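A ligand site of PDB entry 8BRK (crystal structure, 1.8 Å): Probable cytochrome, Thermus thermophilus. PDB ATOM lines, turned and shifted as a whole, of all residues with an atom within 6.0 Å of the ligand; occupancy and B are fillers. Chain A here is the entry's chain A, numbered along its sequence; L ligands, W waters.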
ATOM      1  N   LYS A  15       7.416  25.155 -12.779  1.00  0.00           N
ATOM      2  CA  LYS A  15       7.339  24.794 -11.347  1.00  0.00           C
ATOM      3  C   LYS A  15       6.666  23.445 -11.192  1.00  0.00           C
ATOM      4  O   LYS A  15       6.036  23.007 -12.119  1.00  0.00           O
ATOM      5  CB  LYS A  15       6.492  25.800 -10.563  1.00  0.00           C
ATOM      6  CG  LYS A  15       5.001  25.761 -10.856  1.00  0.00           C
ATOM      7  CD  LYS A  15       4.198  26.703  -9.988  1.00  0.00           C
ATOM      8  CE  LYS A  15       4.110  26.185  -8.566  1.00  0.00           C
ATOM      9  NZ  LYS A  15       3.246  27.062  -7.747  1.00  0.00           N
ATOM     10  N   SER A  16       6.711  22.914  -9.987  1.00  0.00           N
ATOM     11  CA  SER A  16       6.045  21.660  -9.622  1.00  0.00           C
ATOM     12  C   SER A  16       5.348  21.888  -8.291  1.00  0.00           C
ATOM     13  O   SER A  16       5.800  22.736  -7.498  1.00  0.00           O
ATOM     14  CB  SER A  16       7.019  20.534  -9.533  1.00  0.00           C
ATOM     15  OG  SER A  16       7.655  20.339 -10.782  1.00  0.00           O
ATOM     16  N   MET A  17       4.307  21.120  -8.045  1.00  0.00           N
ATOM     17  CA  MET A  17       3.565  21.171  -6.777  1.00  0.00           C
ATOM     18  C   MET A  17       2.781  19.868  -6.646  1.00  0.00           C
ATOM     19  O   MET A  17       2.235  19.401  -7.654  1.00  0.00           O
ATOM     20  CB  MET A  17       2.625  22.355  -6.831  1.00  0.00           C
ATOM     21  CG  MET A  17       1.973  22.697  -5.542  1.00  0.00           C
ATOM     22  SD  MET A  17       0.892  24.115  -5.817  1.00  0.00           S
ATOM     23  CE  MET A  17       0.436  24.457  -4.126  1.00  0.00           C
ATOM     24  N   LEU A  25      -8.470  21.601  -4.012  1.00  0.00           N
ATOM     25  CA  LEU A  25      -8.426  21.212  -5.454  1.00  0.00           C
ATOM     26  C   LEU A  25      -8.090  19.725  -5.605  1.00  0.00           C
ATOM     27  O   LEU A  25      -7.791  19.326  -6.730  1.00  0.00           O
ATOM     28  CB  LEU A  25      -7.359  22.052  -6.162  1.00  0.00           C
ATOM     29  CG  LEU A  25      -7.686  23.531  -6.317  1.00  0.00           C
ATOM     30  CD1 LEU A  25      -6.605  24.227  -7.088  1.00  0.00           C
ATOM     31  CD2 LEU A  25      -9.010  23.703  -7.034  1.00  0.00           C
ATOM     32  N   PHE A  29      -7.686  17.970  -9.174  1.00  0.00           N
ATOM     33  CA  PHE A  29      -6.277  18.167  -9.588  1.00  0.00           C
ATOM     34  C   PHE A  29      -5.299  17.543  -8.597  1.00  0.00           C
ATOM     35  O   PHE A  29      -4.081  17.936  -8.572  1.00  0.00           O
ATOM     36  CB  PHE A  29      -5.941  19.655  -9.767  1.00  0.00           C
ATOM     37  CG  PHE A  29      -6.677  20.385 -10.866  1.00  0.00           C
ATOM     38  CD1 PHE A  29      -6.912  19.787 -12.095  1.00  0.00           C
ATOM     39  CD2 PHE A  29      -7.090  21.683 -10.670  1.00  0.00           C
ATOM     40  CE1 PHE A  29      -7.582  20.468 -13.098  1.00  0.00           C
ATOM     41  CE2 PHE A  29      -7.738  22.381 -11.681  1.00  0.00           C
ATOM     42  CZ  PHE A  29      -7.998  21.763 -12.893  1.00  0.00           C
ATOM     43  N   HIS A  33       1.742  17.872  -9.979  1.00  0.00           N
ATOM     44  CA  HIS A  33       1.687  18.533 -11.285  1.00  0.00           C
ATOM     45  C   HIS A  33       2.972  19.289 -11.582  1.00  0.00           C
ATOM     46  O   HIS A  33       3.652  19.819 -10.681  1.00  0.00           O
ATOM     47  CB  HIS A  33       0.431  19.379 -11.429  1.00  0.00           C
ATOM     48  CG  HIS A  33       0.411  20.635 -10.604  1.00  0.00           C
ATOM     49  ND1 HIS A  33      -0.312  20.725  -9.428  1.00  0.00           N
ATOM     50  CD2 HIS A  33       0.942  21.849 -10.842  1.00  0.00           C
ATOM     51  CE1 HIS A  33      -0.244  21.951  -8.969  1.00  0.00           C
ATOM     52  NE2 HIS A  33       0.534  22.668  -9.820  1.00  0.00           N
ATOM     53  N   ILE A  35       4.222  22.366 -14.402  1.00  0.00           N
ATOM     54  CA  ILE A  35       3.778  23.388 -15.370  1.00  0.00           C
ATOM     55  C   ILE A  35       4.912  23.624 -16.380  1.00  0.00           C
ATOM     56  O   ILE A  35       6.099  23.737 -15.966  1.00  0.00           O
ATOM     57  CB  ILE A  35       3.284  24.624 -14.614  1.00  0.00           C
ATOM     58  CG1 ILE A  35       2.032  24.284 -13.801  1.00  0.00           C
ATOM     59  CG2 ILE A  35       3.030  25.772 -15.565  1.00  0.00           C
ATOM     60  CD1 ILE A  35       1.675  25.303 -12.774  1.00  0.00           C
ATOM     61  N   TYR A  45       6.865  35.207 -17.963  1.00  0.00           N
ATOM     62  CA  TYR A  45       7.123  34.535 -16.666  1.00  0.00           C
ATOM     63  C   TYR A  45       8.418  35.057 -16.063  1.00  0.00           C
ATOM     64  O   TYR A  45       8.435  35.305 -14.847  1.00  0.00           O
ATOM     65  CB  TYR A  45       7.291  33.027 -16.853  1.00  0.00           C
ATOM     66  CG  TYR A  45       6.067  32.176 -16.639  1.00  0.00           C
ATOM     67  CD1 TYR A  45       5.487  32.063 -15.387  1.00  0.00           C
ATOM     68  CD2 TYR A  45       5.477  31.479 -17.675  1.00  0.00           C
ATOM     69  CE1 TYR A  45       4.376  31.271 -15.176  1.00  0.00           C
ATOM     70  CE2 TYR A  45       4.378  30.648 -17.485  1.00  0.00           C
ATOM     71  CZ  TYR A  45       3.848  30.519 -16.210  1.00  0.00           C
ATOM     72  OH  TYR A  45       2.781  29.703 -15.935  1.00  0.00           O
ATOM     73  N   ILE A  59       0.550  27.226 -22.168  1.00  0.00           N
ATOM     74  CA  ILE A  59       0.938  26.760 -20.822  1.00  0.00           C
ATOM     75  C   ILE A  59       0.242  25.424 -20.602  1.00  0.00           C
ATOM     76  O   ILE A  59      -0.980  25.330 -20.852  1.00  0.00           O
ATOM     77  CB  ILE A  59       0.585  27.788 -19.744  1.00  0.00           C
ATOM     78  CG1 ILE A  59       1.018  29.198 -20.145  1.00  0.00           C
ATOM     79  CG2 ILE A  59       1.149  27.341 -18.416  1.00  0.00           C
ATOM     80  CD1 ILE A  59       0.710  30.265 -19.115  1.00  0.00           C
ATOM     81  N   VAL A  60       1.004  24.457 -20.109  1.00  0.00           N
ATOM     82  CA  VAL A  60       0.515  23.074 -19.865  1.00  0.00           C
ATOM     83  C   VAL A  60       0.664  22.775 -18.383  1.00  0.00           C
ATOM     84  O   VAL A  60       1.745  23.039 -17.790  1.00  0.00           O
ATOM     85  CB  VAL A  60       1.229  22.042 -20.755  1.00  0.00           C
ATOM     86  CG1 VAL A  60       0.815  20.630 -20.426  1.00  0.00           C
ATOM     87  CG2 VAL A  60       0.935  22.355 -22.217  1.00  0.00           C
ATOM     88  N   PHE A  61      -0.447  22.308 -17.829  1.00  0.00           N
ATOM     89  CA  PHE A  61      -0.559  21.741 -16.468  1.00  0.00           C
ATOM     90  C   PHE A  61      -0.562  20.230 -16.640  1.00  0.00           C
ATOM     91  O   PHE A  61      -1.546  19.684 -17.194  1.00  0.00           O
ATOM     92  CB  PHE A  61      -1.847  22.288 -15.855  1.00  0.00           C
ATOM     93  CG  PHE A  61      -2.106  21.880 -14.430  1.00  0.00           C
ATOM     94  CD1 PHE A  61      -2.637  20.634 -14.137  1.00  0.00           C
ATOM     95  CD2 PHE A  61      -1.902  22.790 -13.397  1.00  0.00           C
ATOM     96  CE1 PHE A  61      -2.935  20.299 -12.834  1.00  0.00           C
ATOM     97  CE2 PHE A  61      -2.226  22.436 -12.099  1.00  0.00           C
ATOM     98  CZ  PHE A  61      -2.701  21.184 -11.822  1.00  0.00           C
ATOM     99  N   GLY A  82      -3.939  19.946 -18.555  1.00  0.00           N
ATOM    100  CA  GLY A  82      -4.716  21.149 -18.802  1.00  0.00           C
ATOM    101  C   GLY A  82      -3.889  22.076 -19.633  1.00  0.00           C
ATOM    102  O   GLY A  82      -2.654  22.110 -19.425  1.00  0.00           O
ATOM    103  N   VAL A  83      -4.534  22.811 -20.515  1.00  0.00           N
ATOM    104  CA  VAL A  83      -3.836  23.742 -21.448  1.00  0.00           C
ATOM    105  C   VAL A  83      -4.535  25.093 -21.394  1.00  0.00           C
ATOM    106  O   VAL A  83      -5.773  25.166 -21.345  1.00  0.00           O
ATOM    107  CB  VAL A  83      -3.784  23.154 -22.863  1.00  0.00           C
ATOM    108  CG1 VAL A  83      -3.009  24.045 -23.830  1.00  0.00           C
ATOM    109  CG2 VAL A  83      -3.227  21.739 -22.859  1.00  0.00           C
ATOM    110  N   MET A  84      -3.732  26.139 -21.346  1.00  0.00           N
ATOM    111  CA  MET A  84      -4.184  27.499 -21.606  1.00  0.00           C
ATOM    112  C   MET A  84      -3.437  28.023 -22.828  1.00  0.00           C
ATOM    113  O   MET A  84      -2.197  28.021 -22.826  1.00  0.00           O
ATOM    114  CB  MET A  84      -3.911  28.377 -20.390  1.00  0.00           C
ATOM    115  CG  MET A  84      -4.923  28.161 -19.315  1.00  0.00           C
ATOM    116  SD  MET A  84      -4.437  28.935 -17.765  1.00  0.00           S
ATOM    117  CE  MET A  84      -4.633  30.675 -18.145  1.00  0.00           C
ATOM    118  N   TYR A  99      -9.041  27.449 -22.851  1.00  0.00           N
ATOM    119  CA  TYR A  99      -8.899  26.396 -21.825  1.00  0.00           C
ATOM    120  C   TYR A  99      -9.255  25.076 -22.462  1.00  0.00           C
ATOM    121  O   TYR A  99     -10.352  24.959 -23.015  1.00  0.00           O
ATOM    122  CB  TYR A  99      -9.782  26.661 -20.605  1.00  0.00           C
ATOM    123  CG  TYR A  99      -9.405  27.896 -19.847  1.00  0.00           C
ATOM    124  CD1 TYR A  99      -9.939  29.128 -20.187  1.00  0.00           C
ATOM    125  CD2 TYR A  99      -8.531  27.836 -18.776  1.00  0.00           C
ATOM    126  CE1 TYR A  99      -9.603  30.276 -19.488  1.00  0.00           C
ATOM    127  CE2 TYR A  99      -8.218  28.962 -18.038  1.00  0.00           C
ATOM    128  CZ  TYR A  99      -8.764  30.188 -18.395  1.00  0.00           C
ATOM    129  OH  TYR A  99      -8.446  31.308 -17.681  1.00  0.00           O
ATOM    130  N   TYR A 100      -8.347  24.115 -22.378  1.00  0.00           N
ATOM    131  CA  TYR A 100      -8.459  22.758 -22.973  1.00  0.00           C
ATOM    132  C   TYR A 100      -7.916  21.745 -21.976  1.00  0.00           C
ATOM    133  O   TYR A 100      -6.984  22.075 -21.197  1.00  0.00           O
ATOM    134  CB  TYR A 100      -7.700  22.701 -24.304  1.00  0.00           C
ATOM    135  CG  TYR A 100      -8.259  23.632 -25.339  1.00  0.00           C
ATOM    136  CD1 TYR A 100      -9.388  23.273 -26.055  1.00  0.00           C
ATOM    137  CD2 TYR A 100      -7.716  24.890 -25.555  1.00  0.00           C
ATOM    138  CE1 TYR A 100      -9.941  24.112 -27.021  1.00  0.00           C
ATOM    139  CE2 TYR A 100      -8.283  25.752 -26.482  1.00  0.00           C
ATOM    140  CZ  TYR A 100      -9.389  25.362 -27.225  1.00  0.00           C
ATOM    141  OH  TYR A 100      -9.940  26.198 -28.147  1.00  0.00           O
ATOM    142  N   ALA A 101      -8.484  20.546 -21.997  1.00  0.00           N
ATOM    143  CA  ALA A 101      -7.947  19.427 -21.203  1.00  0.00           C
ATOM    144  C   ALA A 101      -7.912  18.160 -22.060  1.00  0.00           C
ATOM    145  O   ALA A 101      -8.742  17.998 -22.986  1.00  0.00           O
ATOM    146  CB  ALA A 101      -8.678  19.269 -19.900  1.00  0.00           C
ATOM    147  N   ILE A 111     -14.920  19.636 -21.016  1.00  0.00           N
ATOM    148  CA  ILE A 111     -14.818  20.542 -19.840  1.00  0.00           C
ATOM    149  C   ILE A 111     -15.715  21.737 -20.146  1.00  0.00           C
ATOM    150  O   ILE A 111     -16.121  21.905 -21.298  1.00  0.00           O
ATOM    151  CB  ILE A 111     -13.337  20.917 -19.589  1.00  0.00           C
ATOM    152  CG1 ILE A 111     -12.709  21.543 -20.838  1.00  0.00           C
ATOM    153  CG2 ILE A 111     -12.583  19.686 -19.145  1.00  0.00           C
ATOM    154  CD1 ILE A 111     -11.678  22.583 -20.562  1.00  0.00           C
ATOM    155  N   ASP A 112     -16.058  22.490 -19.115  1.00  0.00           N
ATOM    156  CA  ASP A 112     -16.644  23.839 -19.281  1.00  0.00           C
ATOM    157  C   ASP A 112     -15.493  24.834 -19.148  1.00  0.00           C
ATOM    158  O   ASP A 112     -14.997  25.079 -18.062  1.00  0.00           O
ATOM    159  CB  ASP A 112     -17.758  24.055 -18.268  1.00  0.00           C
ATOM    160  CG  ASP A 112     -18.426  25.393 -18.422  1.00  0.00           C
ATOM    161  OD1 ASP A 112     -18.083  26.099 -19.393  1.00  0.00           O
ATOM    162  OD2 ASP A 112     -19.300  25.683 -17.587  1.00  0.00           O
ATOM    163  N   PRO A 113     -14.980  25.384 -20.265  1.00  0.00           N
ATOM    164  CA  PRO A 113     -13.898  26.348 -20.203  1.00  0.00           C
ATOM    165  C   PRO A 113     -14.259  27.528 -19.296  1.00  0.00           C
ATOM    166  O   PRO A 113     -13.364  28.065 -18.699  1.00  0.00           O
ATOM    167  CB  PRO A 113     -13.633  26.788 -21.648  1.00  0.00           C
ATOM    168  CG  PRO A 113     -14.773  26.205 -22.456  1.00  0.00           C
ATOM    169  CD  PRO A 113     -15.385  25.066 -21.652  1.00  0.00           C
ATOM    170  N   ALA A 115     -15.893  27.463 -16.495  1.00  0.00           N
ATOM    171  CA  ALA A 115     -15.623  27.005 -15.121  1.00  0.00           C
ATOM    172  C   ALA A 115     -14.106  27.077 -14.840  1.00  0.00           C
ATOM    173  O   ALA A 115     -13.701  27.504 -13.740  1.00  0.00           O
ATOM    174  CB  ALA A 115     -16.200  25.624 -14.933  1.00  0.00           C
ATOM    175  N   CYS A 116     -13.261  26.704 -15.798  1.00  0.00           N
ATOM    176  CA  CYS A 116     -11.793  26.920 -15.660  1.00  0.00           C
ATOM    177  C   CYS A 116     -11.535  28.402 -15.428  1.00  0.00           C
ATOM    178  O   CYS A 116     -10.851  28.772 -14.429  1.00  0.00           O
ATOM    179  CB  CYS A 116     -10.998  26.504 -16.903  1.00  0.00           C
ATOM    180  SG  CYS A 116     -11.342  24.875 -17.508  1.00  0.00           S
ATOM    181  N   HIS A 117     -12.071  29.245 -16.318  1.00  0.00           N
ATOM    182  CA  HIS A 117     -11.842  30.705 -16.298  1.00  0.00           C
ATOM    183  C   HIS A 117     -12.340  31.296 -14.979  1.00  0.00           C
ATOM    184  O   HIS A 117     -11.710  32.238 -14.503  1.00  0.00           O
ATOM    185  CB  HIS A 117     -12.567  31.398 -17.441  1.00  0.00           C
ATOM    186  CG  HIS A 117     -12.127  32.821 -17.585  1.00  0.00           C
ATOM    187  ND1 HIS A 117     -10.807  33.131 -17.805  1.00  0.00           N
ATOM    188  CD2 HIS A 117     -12.818  33.980 -17.534  1.00  0.00           C
ATOM    189  CE1 HIS A 117     -10.694  34.450 -17.861  1.00  0.00           C
ATOM    190  NE2 HIS A 117     -11.921  34.984 -17.719  1.00  0.00           N
ATOM    191  N   CYS A 119     -12.418  30.286 -11.951  1.00  0.00           N
ATOM    192  CA  CYS A 119     -11.360  30.167 -10.914  1.00  0.00           C
ATOM    193  C   CYS A 119     -10.150  31.027 -11.289  1.00  0.00           C
ATOM    194  O   CYS A 119      -9.640  31.733 -10.415  1.00  0.00           O
ATOM    195  CB  CYS A 119     -10.952  28.720 -10.728  1.00  0.00           C
ATOM    196  SG  CYS A 119      -9.850  28.583  -9.353  1.00  0.00           S
ATOM    197  N   HIS A 120      -9.704  30.990 -12.535  1.00  0.00           N
ATOM    198  CA  HIS A 120      -8.509  31.762 -13.007  1.00  0.00           C
ATOM    199  C   HIS A 120      -8.725  33.272 -12.939  1.00  0.00           C
ATOM    200  O   HIS A 120      -7.709  34.026 -12.894  1.00  0.00           O
ATOM    201  CB  HIS A 120      -8.092  31.282 -14.404  1.00  0.00           C
ATOM    202  CG  HIS A 120      -7.276  30.042 -14.349  1.00  0.00           C
ATOM    203  ND1 HIS A 120      -5.907  30.064 -14.471  1.00  0.00           N
ATOM    204  CD2 HIS A 120      -7.607  28.760 -14.076  1.00  0.00           C
ATOM    205  CE1 HIS A 120      -5.441  28.841 -14.335  1.00  0.00           C
ATOM    206  NE2 HIS A 120      -6.457  28.017 -14.090  1.00  0.00           N
ATOM    207  N   TYR A 128      -4.496  35.973 -15.590  1.00  0.00           N
ATOM    208  CA  TYR A 128      -5.273  34.738 -15.349  1.00  0.00           C
ATOM    209  C   TYR A 128      -4.352  33.542 -15.102  1.00  0.00           C
ATOM    210  O   TYR A 128      -4.850  32.406 -15.106  1.00  0.00           O
ATOM    211  CB  TYR A 128      -6.246  34.521 -16.509  1.00  0.00           C
ATOM    212  CG  TYR A 128      -7.140  35.708 -16.726  1.00  0.00           C
ATOM    213  CD1 TYR A 128      -8.212  35.949 -15.870  1.00  0.00           C
ATOM    214  CD2 TYR A 128      -6.875  36.647 -17.714  1.00  0.00           C
ATOM    215  CE1 TYR A 128      -9.031  37.048 -16.026  1.00  0.00           C
ATOM    216  CE2 TYR A 128      -7.708  37.751 -17.897  1.00  0.00           C
ATOM    217  CZ  TYR A 128      -8.780  37.955 -17.043  1.00  0.00           C
ATOM    218  OH  TYR A 128      -9.567  39.064 -17.195  1.00  0.00           O
ATOM    219  N   VAL A 129      -3.067  33.786 -14.873  1.00  0.00           N
ATOM    220  CA  VAL A 129      -2.056  32.732 -14.617  1.00  0.00           C
ATOM    221  C   VAL A 129      -1.633  32.829 -13.151  1.00  0.00           C
ATOM    222  O   VAL A 129      -1.153  33.877 -12.723  1.00  0.00           O
ATOM    223  CB  VAL A 129      -0.880  32.858 -15.598  1.00  0.00           C
ATOM    224  CG1 VAL A 129       0.233  31.896 -15.257  1.00  0.00           C
ATOM    225  CG2 VAL A 129      -1.345  32.614 -17.035  1.00  0.00           C
ATOM    226  N   PHE A 130      -1.855  31.737 -12.411  1.00  0.00           N
ATOM    227  CA  PHE A 130      -1.509  31.654 -10.976  1.00  0.00           C
ATOM    228  C   PHE A 130      -0.017  31.492 -10.773  1.00  0.00           C
ATOM    229  O   PHE A 130       0.561  32.176  -9.917  1.00  0.00           O
ATOM    230  CB  PHE A 130      -2.235  30.463 -10.347  1.00  0.00           C
ATOM    231  CG  PHE A 130      -3.718  30.690 -10.182  1.00  0.00           C
ATOM    232  CD1 PHE A 130      -4.196  31.520  -9.170  1.00  0.00           C
ATOM    233  CD2 PHE A 130      -4.619  30.049 -11.003  1.00  0.00           C
ATOM    234  CE1 PHE A 130      -5.555  31.730  -9.034  1.00  0.00           C
ATOM    235  CE2 PHE A 130      -5.984  30.198 -10.813  1.00  0.00           C
ATOM    236  CZ  PHE A 130      -6.447  31.055  -9.831  1.00  0.00           C
ATOM    237  N   SER A 131       0.577  30.540 -11.494  1.00  0.00           N
ATOM    238  CA  SER A 131       1.935  30.009 -11.245  1.00  0.00           C
ATOM    239  C   SER A 131       2.969  31.108 -11.467  1.00  0.00           C
ATOM    240  O   SER A 131       2.745  31.944 -12.347  1.00  0.00           O
ATOM    241  CB  SER A 131       2.236  28.805 -12.116  1.00  0.00           C
ATOM    242  OG  SER A 131       2.000  29.111 -13.469  1.00  0.00           O
ATOM    243  N   ALA A 132       4.051  31.087 -10.701  1.00  0.00           N
ATOM    244  CA  ALA A 132       5.227  31.943 -10.931  1.00  0.00           C
ATOM    245  C   ALA A 132       6.389  31.025 -11.316  1.00  0.00           C
ATOM    246  O   ALA A 132       6.437  29.857 -10.880  1.00  0.00           O
ATOM    247  CB  ALA A 132       5.539  32.774  -9.707  1.00  0.00           C
HETATM  248 FE1  LIG L   1      -6.212  25.948 -13.480  1.00  0.00          FE
HETATM  249  C1  LIG L   1      -2.919  26.441 -12.946  1.00  0.00           C
HETATM  250  C2  LIG L   1      -5.579  25.046 -16.768  1.00  0.00           C
HETATM  251  C3  LIG L   1      -9.454  24.968 -13.811  1.00  0.00           C
HETATM  252  C4  LIG L   1      -6.884  26.746 -10.191  1.00  0.00           C
HETATM  253  N1  LIG L   1      -4.538  25.757 -14.674  1.00  0.00           N
HETATM  254  C5  LIG L   1      -3.316  26.126 -14.306  1.00  0.00           C
HETATM  255  C6  LIG L   1      -2.333  26.019 -15.381  1.00  0.00           C
HETATM  256  C7  LIG L   1      -3.116  25.632 -16.549  1.00  0.00           C
HETATM  257  C8  LIG L   1      -4.454  25.467 -15.960  1.00  0.00           C
HETATM  258  C9  LIG L   1      -2.657  25.334 -17.949  1.00  0.00           C
HETATM  259  C10 LIG L   1      -0.911  26.383 -15.304  1.00  0.00           C
HETATM  260  C11 LIG L   1      -1.033  27.934 -15.515  1.00  0.00           C
HETATM  261  C12 LIG L   1      -1.389  28.764 -14.265  1.00  0.00           C
HETATM  262  O1  LIG L   1      -2.430  29.456 -14.175  1.00  0.00           O
HETATM  263  O2  LIG L   1      -0.597  28.781 -13.296  1.00  0.00           O
HETATM  264  N2  LIG L   1      -7.321  25.157 -14.994  1.00  0.00           N
HETATM  265  C13 LIG L   1      -6.925  24.820 -16.251  1.00  0.00           C
HETATM  266  C14 LIG L   1      -7.947  24.269 -17.105  1.00  0.00           C
HETATM  267  C15 LIG L   1      -9.084  24.265 -16.187  1.00  0.00           C
HETATM  268  C16 LIG L   1      -8.591  24.817 -14.949  1.00  0.00           C
HETATM  269  C17 LIG L   1      -7.753  23.851 -18.537  1.00  0.00           C
HETATM  270  C18 LIG L   1     -10.479  23.782 -16.459  1.00  0.00           C
HETATM  271  C19 LIG L   1     -10.477  22.389 -16.981  1.00  0.00           C
HETATM  272  N3  LIG L   1      -7.876  25.892 -12.254  1.00  0.00           N
HETATM  273  C20 LIG L   1      -9.105  25.510 -12.551  1.00  0.00           C
HETATM  274  C21 LIG L   1     -10.130  25.627 -11.509  1.00  0.00           C
HETATM  275  C22 LIG L   1      -9.335  26.198 -10.447  1.00  0.00           C
HETATM  276  C23 LIG L   1      -7.988  26.304 -11.010  1.00  0.00           C
HETATM  277  C24 LIG L   1     -11.585  25.273 -11.674  1.00  0.00           C
HETATM  278  C25 LIG L   1      -9.733  26.738  -9.123  1.00  0.00           C
HETATM  279  C26 LIG L   1     -10.964  26.115  -8.538  1.00  0.00           C
HETATM  280  N4  LIG L   1      -5.068  26.448 -11.817  1.00  0.00           N
HETATM  281  C27 LIG L   1      -5.481  26.711 -10.584  1.00  0.00           C
HETATM  282  C28 LIG L   1      -4.382  27.036  -9.654  1.00  0.00           C
HETATM  283  C29 LIG L   1      -3.189  26.932 -10.480  1.00  0.00           C
HETATM  284  C30 LIG L   1      -3.746  26.528 -11.775  1.00  0.00           C
HETATM  285  C31 LIG L   1      -4.463  27.401  -8.235  1.00  0.00           C
HETATM  286  C32 LIG L   1      -1.778  27.125 -10.076  1.00  0.00           C
HETATM  287  C33 LIG L   1      -1.118  25.783  -9.711  1.00  0.00           C
HETATM  288  C34 LIG L   1       0.358  25.973  -9.296  1.00  0.00           C
HETATM  289  O3  LIG L   1       1.177  25.006  -9.304  1.00  0.00           O
HETATM  290  O4  LIG L   1       0.753  27.075  -8.901  1.00  0.00           O
HETATM  291  O   HOH W   1     -12.819  23.020 -13.931  1.00  0.00           O
HETATM  292  O   HOH W   2      -0.993  28.704  -7.057  1.00  0.00           O
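SG of Cys 116 is bonded to C18 of the ligand, 1.7 Å away. SG of Cys 119 is bonded to C25 of the ligand, 1.9 Å away. A ring nitrogen (NE2) of His 120 binds an iron atom (FE1) of the ligand, at 2.2 Å. A ring nitrogen (NE2) of His 33 lies within hydrogen-bond range of an oxygen (O3) of the ligand. N of Ser 131 is in hydrogen-bond range of O2 of the ligand (2.8 Å). O2 of the ligand sits at hydrogen-bond distance from OG of Ser 131. An oxygen (O4) of the ligand lies within salt-bridge range of the side-chain amino group of Lys 15 (2.7 Å). The backbone NH (N) of Phe 130 lies within hydrogen-bond range of an oxygen (O1) of the ligand, at 2.9 Å.
An oxygen (O3) of the ligand sits close to the side-chain sulfur of Met 17, 3.6 Å away. CD2 of Leu 25 touches C26 of the ligand, 3.4 Å away. Phe 29 touches the ligand. Ile 35 touches the ligand (CD1 to O3, 3.5 Å). Ile 59 touches the ligand (O to C9, 3.4 Å). CB of Phe 61 touches C7 of the ligand, 3.6 Å away. Gly 82 touches the ligand. Val 83 touches the ligand (O to C17, 3.7 Å). N of Met 84 touches C9 of the ligand (3.7 Å). Tyr 99 touches the ligand (CD2 to C14, 3.98 Å). Tyr 100 touches the ligand (O to C17, 3.3 Å). Ile 111 touches the ligand. Ala 115 touches the ligand (O to C24, 3.7 Å). Tyr 128 touches the ligand (O to O1, 3.9 Å). Val 129 touches the ligand (CA to O1, 3.3 Å). Hydrophobic or aromatic side chains that line the ligand: Met 17, Leu 25, Phe 29, His 33, Ile 35, Ile 59, Phe 61, Met 84, Tyr 99, Ile 111, His 120, Val 129 and Phe 130. 22 residues have an atom within 4 Å of the ligand: Lys 15, Met 17, Leu 25, Phe 29, His 33, Ile 35, Ile 59, Phe 61, Gly 82, Val 83, Met 84, Tyr 99, Tyr 100, Ile 111, Ala 115, Cys 116, Cys 119, His 120, Tyr 128, Val 129, Phe 130 and Ser 131.
The side-chain sulfur of Met 84 lies close to a ring nitrogen (ND1) of His 120 (3.8 Å). A ring nitrogen (ND1) of His 120 sits at hydrogen-bond distance from the backbone carbonyl oxygen (O) of Tyr 128 (2.6 Å). N of His 33 is in hydrogen-bond range of O of Met 17, 2.8 Å away. The backbone NH of Ile 35 sits at hydrogen-bond distance from the backbone carbonyl oxygen of Lys 15, 3.0 Å away. The backbone NH (N) of Val 83 sits at hydrogen-bond distance from the backbone carbonyl oxygen (O) of Tyr 100 (2.6 Å). The backbone carbonyl oxygen (O) of Ile 59 lies within hydrogen-bond range of the backbone NH (N) of Met 84 (2.9 Å). The backbone carbonyl oxygen (O) of Gly 82 lies within hydrogen-bond range of the backbone NH (N) of Phe 61, 2.7 Å away. OH of Tyr 99 is in hydrogen-bond range of ND1 of His 117 (3.0 Å).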
